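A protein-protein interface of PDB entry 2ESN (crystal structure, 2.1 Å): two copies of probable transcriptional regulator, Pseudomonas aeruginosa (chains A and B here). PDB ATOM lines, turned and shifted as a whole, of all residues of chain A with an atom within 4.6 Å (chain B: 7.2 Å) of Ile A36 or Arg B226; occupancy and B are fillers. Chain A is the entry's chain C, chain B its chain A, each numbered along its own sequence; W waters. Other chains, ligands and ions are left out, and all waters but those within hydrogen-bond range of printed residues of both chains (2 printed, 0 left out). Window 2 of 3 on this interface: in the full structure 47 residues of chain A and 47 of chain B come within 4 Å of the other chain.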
ATOM      1  N   GLY A  28      -3.434  25.822 -35.576  1.00  0.00           N
ATOM      2  CA  GLY A  28      -2.319  25.948 -34.597  1.00  0.00           C
ATOM      3  C   GLY A  28      -2.695  26.832 -33.389  1.00  0.00           C
ATOM      4  O   GLY A  28      -2.569  26.407 -32.274  1.00  0.00           O
ATOM      5  N   ALA A  31      -5.643  25.215 -31.421  1.00  0.00           N
ATOM      6  CA  ALA A  31      -5.161  24.052 -30.625  1.00  0.00           C
ATOM      7  C   ALA A  31      -4.419  24.602 -29.383  1.00  0.00           C
ATOM      8  O   ALA A  31      -4.602  24.085 -28.265  1.00  0.00           O
ATOM      9  CB  ALA A  31      -4.170  23.179 -31.507  1.00  0.00           C
ATOM     10  N   SER A  32      -3.586  25.658 -29.560  1.00  0.00           N
ATOM     11  CA  SER A  32      -2.921  26.236 -28.391  1.00  0.00           C
ATOM     12  C   SER A  32      -3.917  26.744 -27.305  1.00  0.00           C
ATOM     13  O   SER A  32      -3.762  26.405 -26.135  1.00  0.00           O
ATOM     14  CB  SER A  32      -2.003  27.357 -28.814  1.00  0.00           C
ATOM     15  OG  SER A  32      -1.562  27.993 -27.639  1.00  0.00           O
ATOM     16  N   LEU A  34      -6.838  25.752 -26.694  1.00  0.00           N
ATOM     17  CA  LEU A  34      -7.540  24.610 -26.150  1.00  0.00           C
ATOM     18  C   LEU A  34      -6.568  23.758 -25.315  1.00  0.00           C
ATOM     19  O   LEU A  34      -6.978  22.832 -24.650  1.00  0.00           O
ATOM     20  CB  LEU A  34      -8.178  23.784 -27.281  1.00  0.00           C
ATOM     21  CG  LEU A  34      -9.476  24.345 -27.846  1.00  0.00           C
ATOM     22  CD1 LEU A  34     -10.127  23.214 -28.453  1.00  0.00           C
ATOM     23  CD2 LEU A  34     -10.356  24.884 -26.762  1.00  0.00           C
ATOM     24  N   ALA A  35      -5.280  24.073 -25.369  1.00  0.00           N
ATOM     25  CA  ALA A  35      -4.264  23.242 -24.749  1.00  0.00           C
ATOM     26  C   ALA A  35      -4.373  21.771 -25.176  1.00  0.00           C
ATOM     27  O   ALA A  35      -4.347  20.858 -24.349  1.00  0.00           O
ATOM     28  CB  ALA A  35      -4.319  23.386 -23.230  1.00  0.00           C
ATOM     29  N   ILE A  36      -4.524  21.526 -26.467  1.00  0.00           N
ATOM     30  CA  ILE A  36      -4.433  20.156 -26.962  1.00  0.00           C
ATOM     31  C   ILE A  36      -3.483  20.227 -28.096  1.00  0.00           C
ATOM     32  O   ILE A  36      -3.137  21.344 -28.548  1.00  0.00           O
ATOM     33  CB  ILE A  36      -5.791  19.618 -27.435  1.00  0.00           C
ATOM     34  CG1 ILE A  36      -6.433  20.522 -28.511  1.00  0.00           C
ATOM     35  CG2 ILE A  36      -6.747  19.472 -26.197  1.00  0.00           C
ATOM     36  CD1 ILE A  36      -7.778  19.891 -29.066  1.00  0.00           C
ATOM     37  N   SER A  37      -3.102  19.063 -28.605  1.00  0.00           N
ATOM     38  CA  SER A  37      -2.103  19.004 -29.659  1.00  0.00           C
ATOM     39  C   SER A  37      -2.765  19.265 -31.034  1.00  0.00           C
ATOM     40  O   SER A  37      -3.984  19.209 -31.178  1.00  0.00           O
ATOM     41  CB  SER A  37      -1.335  17.668 -29.596  1.00  0.00           C
ATOM     42  OG  SER A  37      -1.897  16.670 -30.471  1.00  0.00           O
ATOM     43  N   ALA A  38      -1.941  19.589 -32.024  1.00  0.00           N
ATOM     44  CA  ALA A  38      -2.389  19.977 -33.349  1.00  0.00           C
ATOM     45  C   ALA A  38      -3.109  18.773 -33.964  1.00  0.00           C
ATOM     46  O   ALA A  38      -4.124  18.869 -34.629  1.00  0.00           O
ATOM     47  CB  ALA A  38      -1.156  20.368 -34.191  1.00  0.00           C
ATOM     48  N   ALA A  40      -4.512  16.026 -32.182  1.00  0.00           N
ATOM     49  CA  ALA A  40      -5.805  15.848 -31.522  1.00  0.00           C
ATOM     50  C   ALA A  40      -6.831  16.879 -32.048  1.00  0.00           C
ATOM     51  O   ALA A  40      -7.954  16.514 -32.365  1.00  0.00           O
ATOM     52  CB  ALA A  40      -5.674  15.918 -30.065  1.00  0.00           C
ATOM     53  N   PHE A  41      -6.447  18.165 -32.148  1.00  0.00           N
ATOM     54  CA  PHE A  41      -7.310  19.215 -32.734  1.00  0.00           C
ATOM     55  C   PHE A  41      -7.756  18.801 -34.129  1.00  0.00           C
ATOM     56  O   PHE A  41      -8.905  18.835 -34.411  1.00  0.00           O
ATOM     57  CB  PHE A  41      -6.613  20.585 -32.787  1.00  0.00           C
ATOM     58  CG  PHE A  41      -7.558  21.732 -33.139  1.00  0.00           C
ATOM     59  CD1 PHE A  41      -8.182  22.464 -32.155  1.00  0.00           C
ATOM     60  CD2 PHE A  41      -7.821  22.063 -34.463  1.00  0.00           C
ATOM     61  CE1 PHE A  41      -9.081  23.508 -32.489  1.00  0.00           C
ATOM     62  CE2 PHE A  41      -8.706  23.119 -34.789  1.00  0.00           C
ATOM     63  CZ  PHE A  41      -9.327  23.812 -33.829  1.00  0.00           C
ATOM     64  N   TYR B 198      12.923  31.501 -24.651  1.00  0.00           N
ATOM     65  CA  TYR B 198      11.786  32.273 -25.135  1.00  0.00           C
ATOM     66  C   TYR B 198      10.449  31.566 -24.796  1.00  0.00           C
ATOM     67  O   TYR B 198       9.542  32.176 -24.227  1.00  0.00           O
ATOM     68  CB  TYR B 198      11.930  32.488 -26.656  1.00  0.00           C
ATOM     69  CG  TYR B 198      10.824  33.278 -27.391  1.00  0.00           C
ATOM     70  CD1 TYR B 198      10.906  34.660 -27.517  1.00  0.00           C
ATOM     71  CD2 TYR B 198       9.704  32.630 -27.949  1.00  0.00           C
ATOM     72  CE1 TYR B 198       9.963  35.357 -28.197  1.00  0.00           C
ATOM     73  CE2 TYR B 198       8.691  33.349 -28.610  1.00  0.00           C
ATOM     74  CZ  TYR B 198       8.847  34.708 -28.743  1.00  0.00           C
ATOM     75  OH  TYR B 198       7.910  35.439 -29.436  1.00  0.00           O
ATOM     76  N   LEU B 199      10.383  30.256 -25.059  1.00  0.00           N
ATOM     77  CA  LEU B 199       9.141  29.507 -24.881  1.00  0.00           C
ATOM     78  C   LEU B 199       8.883  29.139 -23.427  1.00  0.00           C
ATOM     79  O   LEU B 199       7.790  28.710 -23.129  1.00  0.00           O
ATOM     80  CB  LEU B 199       9.133  28.236 -25.763  1.00  0.00           C
ATOM     81  CG  LEU B 199       9.246  28.511 -27.266  1.00  0.00           C
ATOM     82  CD1 LEU B 199       9.329  27.223 -27.993  1.00  0.00           C
ATOM     83  CD2 LEU B 199       8.038  29.339 -27.802  1.00  0.00           C
ATOM     84  N   ALA B 200       9.888  29.334 -22.553  1.00  0.00           N
ATOM     85  CA  ALA B 200       9.792  29.135 -21.090  1.00  0.00           C
ATOM     86  C   ALA B 200       9.250  30.373 -20.345  1.00  0.00           C
ATOM     87  O   ALA B 200       8.930  30.319 -19.172  1.00  0.00           O
ATOM     88  CB  ALA B 200      11.173  28.780 -20.553  1.00  0.00           C
ATOM     89  N   HIS B 203       4.233  35.684 -22.463  1.00  0.00           N
ATOM     90  CA  HIS B 203       4.382  36.679 -23.466  1.00  0.00           C
ATOM     91  C   HIS B 203       3.277  37.741 -23.489  1.00  0.00           C
ATOM     92  O   HIS B 203       2.136  37.457 -23.194  1.00  0.00           O
ATOM     93  CB  HIS B 203       4.444  36.018 -24.830  1.00  0.00           C
ATOM     94  CG  HIS B 203       5.634  35.116 -24.964  1.00  0.00           C
ATOM     95  ND1 HIS B 203       6.759  35.467 -25.687  1.00  0.00           N
ATOM     96  CD2 HIS B 203       5.884  33.899 -24.431  1.00  0.00           C
ATOM     97  CE1 HIS B 203       7.650  34.495 -25.592  1.00  0.00           C
ATOM     98  NE2 HIS B 203       7.149  33.535 -24.836  1.00  0.00           N
ATOM     99  N   ASP B 217       2.222  34.427 -32.933  1.00  0.00           N
ATOM    100  CA  ASP B 217       1.651  33.089 -32.648  1.00  0.00           C
ATOM    101  C   ASP B 217       1.391  32.247 -33.953  1.00  0.00           C
ATOM    102  O   ASP B 217       1.572  31.018 -33.986  1.00  0.00           O
ATOM    103  CB  ASP B 217       0.357  33.283 -31.878  1.00  0.00           C
ATOM    104  CG  ASP B 217       0.606  33.943 -30.520  1.00  0.00           C
ATOM    105  OD1 ASP B 217       0.157  35.083 -30.306  1.00  0.00           O
ATOM    106  OD2 ASP B 217       1.353  33.352 -29.713  1.00  0.00           O
ATOM    107  N   LEU B 220       4.728  31.115 -35.365  1.00  0.00           N
ATOM    108  CA  LEU B 220       5.180  29.966 -34.572  1.00  0.00           C
ATOM    109  C   LEU B 220       4.406  28.662 -34.847  1.00  0.00           C
ATOM    110  O   LEU B 220       4.995  27.575 -34.839  1.00  0.00           O
ATOM    111  CB  LEU B 220       5.237  30.285 -33.077  1.00  0.00           C
ATOM    112  CG  LEU B 220       6.306  31.392 -32.718  1.00  0.00           C
ATOM    113  CD1 LEU B 220       6.172  31.871 -31.277  1.00  0.00           C
ATOM    114  CD2 LEU B 220       7.692  30.800 -32.907  1.00  0.00           C
ATOM    115  N   ALA B 221       3.097  28.759 -35.013  1.00  0.00           N
ATOM    116  CA  ALA B 221       2.257  27.590 -35.242  1.00  0.00           C
ATOM    117  C   ALA B 221       2.653  26.870 -36.567  1.00  0.00           C
ATOM    118  O   ALA B 221       2.519  25.654 -36.654  1.00  0.00           O
ATOM    119  CB  ALA B 221       0.825  28.005 -35.294  1.00  0.00           C
ATOM    120  N   SER B 223       5.537  26.301 -37.590  1.00  0.00           N
ATOM    121  CA  SER B 223       6.551  25.340 -37.189  1.00  0.00           C
ATOM    122  C   SER B 223       6.141  24.412 -36.117  1.00  0.00           C
ATOM    123  O   SER B 223       7.021  23.758 -35.589  1.00  0.00           O
ATOM    124  CB  SER B 223       7.809  25.996 -36.656  1.00  0.00           C
ATOM    125  OG  SER B 223       8.272  26.933 -37.573  1.00  0.00           O
ATOM    126  N   GLY B 224       4.856  24.273 -35.807  1.00  0.00           N
ATOM    127  CA  GLY B 224       4.508  23.369 -34.679  1.00  0.00           C
ATOM    128  C   GLY B 224       4.902  23.916 -33.297  1.00  0.00           C
ATOM    129  O   GLY B 224       4.969  23.162 -32.321  1.00  0.00           O
ATOM    130  N   LEU B 225       5.125  25.228 -33.180  1.00  0.00           N
ATOM    131  CA  LEU B 225       5.464  25.809 -31.847  1.00  0.00           C
ATOM    132  C   LEU B 225       4.371  26.708 -31.221  1.00  0.00           C
ATOM    133  O   LEU B 225       3.559  27.337 -31.941  1.00  0.00           O
ATOM    134  CB  LEU B 225       6.765  26.622 -31.956  1.00  0.00           C
ATOM    135  CG  LEU B 225       8.057  25.907 -32.406  1.00  0.00           C
ATOM    136  CD1 LEU B 225       9.090  26.935 -32.575  1.00  0.00           C
ATOM    137  CD2 LEU B 225       8.510  24.917 -31.388  1.00  0.00           C
ATOM    138  N   ARG B 226       4.363  26.813 -29.903  1.00  0.00           N
ATOM    139  CA  ARG B 226       3.457  27.774 -29.298  1.00  0.00           C
ATOM    140  C   ARG B 226       4.022  28.419 -28.086  1.00  0.00           C
ATOM    141  O   ARG B 226       4.896  27.854 -27.434  1.00  0.00           O
ATOM    142  CB  ARG B 226       2.095  27.200 -28.906  1.00  0.00           C
ATOM    143  CG  ARG B 226       2.091  25.952 -28.184  1.00  0.00           C
ATOM    144  CD  ARG B 226       1.151  25.106 -29.061  1.00  0.00           C
ATOM    145  NE  ARG B 226       0.225  24.436 -28.203  1.00  0.00           N
ATOM    146  CZ  ARG B 226      -0.618  23.484 -28.550  1.00  0.00           C
ATOM    147  NH1 ARG B 226      -0.739  23.062 -29.799  1.00  0.00           N
ATOM    148  NH2 ARG B 226      -1.352  22.978 -27.592  1.00  0.00           N
ATOM    149  N   ARG B 227       3.508  29.601 -27.812  1.00  0.00           N
ATOM    150  CA  ARG B 227       3.965  30.331 -26.638  1.00  0.00           C
ATOM    151  C   ARG B 227       2.856  30.536 -25.605  1.00  0.00           C
ATOM    152  O   ARG B 227       1.680  30.524 -25.919  1.00  0.00           O
ATOM    153  CB  ARG B 227       4.687  31.616 -27.057  1.00  0.00           C
ATOM    154  CG  ARG B 227       3.861  32.567 -27.726  1.00  0.00           C
ATOM    155  CD  ARG B 227       4.748  33.715 -28.384  1.00  0.00           C
ATOM    156  NE  ARG B 227       3.730  34.578 -29.037  1.00  0.00           N
ATOM    157  CZ  ARG B 227       3.852  35.825 -29.456  1.00  0.00           C
ATOM    158  NH1 ARG B 227       5.011  36.458 -29.310  1.00  0.00           N
ATOM    159  NH2 ARG B 227       2.779  36.420 -30.029  1.00  0.00           N
ATOM    160  N   GLU B 228       3.240  30.694 -24.353  1.00  0.00           N
ATOM    161  CA  GLU B 228       2.270  30.950 -23.330  1.00  0.00           C
ATOM    162  C   GLU B 228       2.027  32.430 -23.307  1.00  0.00           C
ATOM    163  O   GLU B 228       2.927  33.209 -23.010  1.00  0.00           O
ATOM    164  CB  GLU B 228       2.815  30.472 -21.969  1.00  0.00           C
ATOM    165  CG  GLU B 228       1.700  30.699 -20.975  1.00  0.00           C
ATOM    166  CD  GLU B 228       1.965  30.220 -19.591  1.00  0.00           C
ATOM    167  OE1 GLU B 228       0.975  30.274 -18.795  1.00  0.00           O
ATOM    168  OE2 GLU B 228       3.126  29.803 -19.316  1.00  0.00           O
ATOM    169  N   VAL B 229       0.801  32.818 -23.607  1.00  0.00           N
ATOM    170  CA  VAL B 229       0.344  34.220 -23.696  1.00  0.00           C
ATOM    171  C   VAL B 229      -0.239  34.702 -22.365  1.00  0.00           C
ATOM    172  O   VAL B 229      -1.184  34.067 -21.793  1.00  0.00           O
ATOM    173  CB  VAL B 229      -0.666  34.374 -24.888  1.00  0.00           C
ATOM    174  CG1 VAL B 229      -1.310  35.788 -24.927  1.00  0.00           C
ATOM    175  CG2 VAL B 229       0.112  34.098 -26.217  1.00  0.00           C
HETATM  176  O   HOH W   1      -0.830  30.504 -28.097  1.00  0.00           O
HETATM  177  O   HOH W   2       0.121  27.826 -25.073  1.00  0.00           O
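Water W1 bridges OG of Ser A32 and O of Arg B227.
Water W2 lies within hydrogen-bond range of the side-chain hydroxyl of Ser A32 and the backbone carbonyl oxygen of Arg B227.
Of the printed residues of chain B, Gly A28 touches Ala B221.
Printed residues of chain B within 4 Å of Ala A31: Arg B226.
Of the printed residues of chain B, Ser A32 touches Arg B226.
Ile A36 touches one residue of chain B.
Of the printed residues of chain A, Ala B221 touches Gly A28.
Arg B226 touches just these residues of chain A: Ala A31 (3.5 Å), Ser A32 (3.6 Å) and Ile A36 (2.6 Å).
The nearest printed residue of chain A that does not touch Ala B221 is Ala A38 (6.9 Å).
Of the 14 printed residues of chain B, 2 touch a printed residue of chain A.
Hydrophobic or aromatic side chains of chain B within 4 Å of the printed part of chain A: Ala B221.
Among the printed residues, no Asp or Glu carboxylate lies within 4 Å of a Lys or Arg side-chain nitrogen of the other chain.
Among the printed residues, merely in contact across the chains: Ser A32 with Arg B226 (3.6 Å) and Gly A28 with Ala B221 (3.8 Å).
The guanidinium group (NH2) of Arg B226 sits at hydrogen-bond distance from the backbone carbonyl oxygen (O) of Ala A31 (3.5 Å).
The guanidinium group (NH2) of Arg B226 lies within hydrogen-bond range of the backbone carbonyl oxygen (O) of Ile A36, 2.6 Å away.
No position is printed for both chains.
Of the 4 pairs that touch across the chains among the printed residues, none has its exchanged pair printed and touching as well.
O of Ala A31 is in hydrogen-bond range of N of Ile A36.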
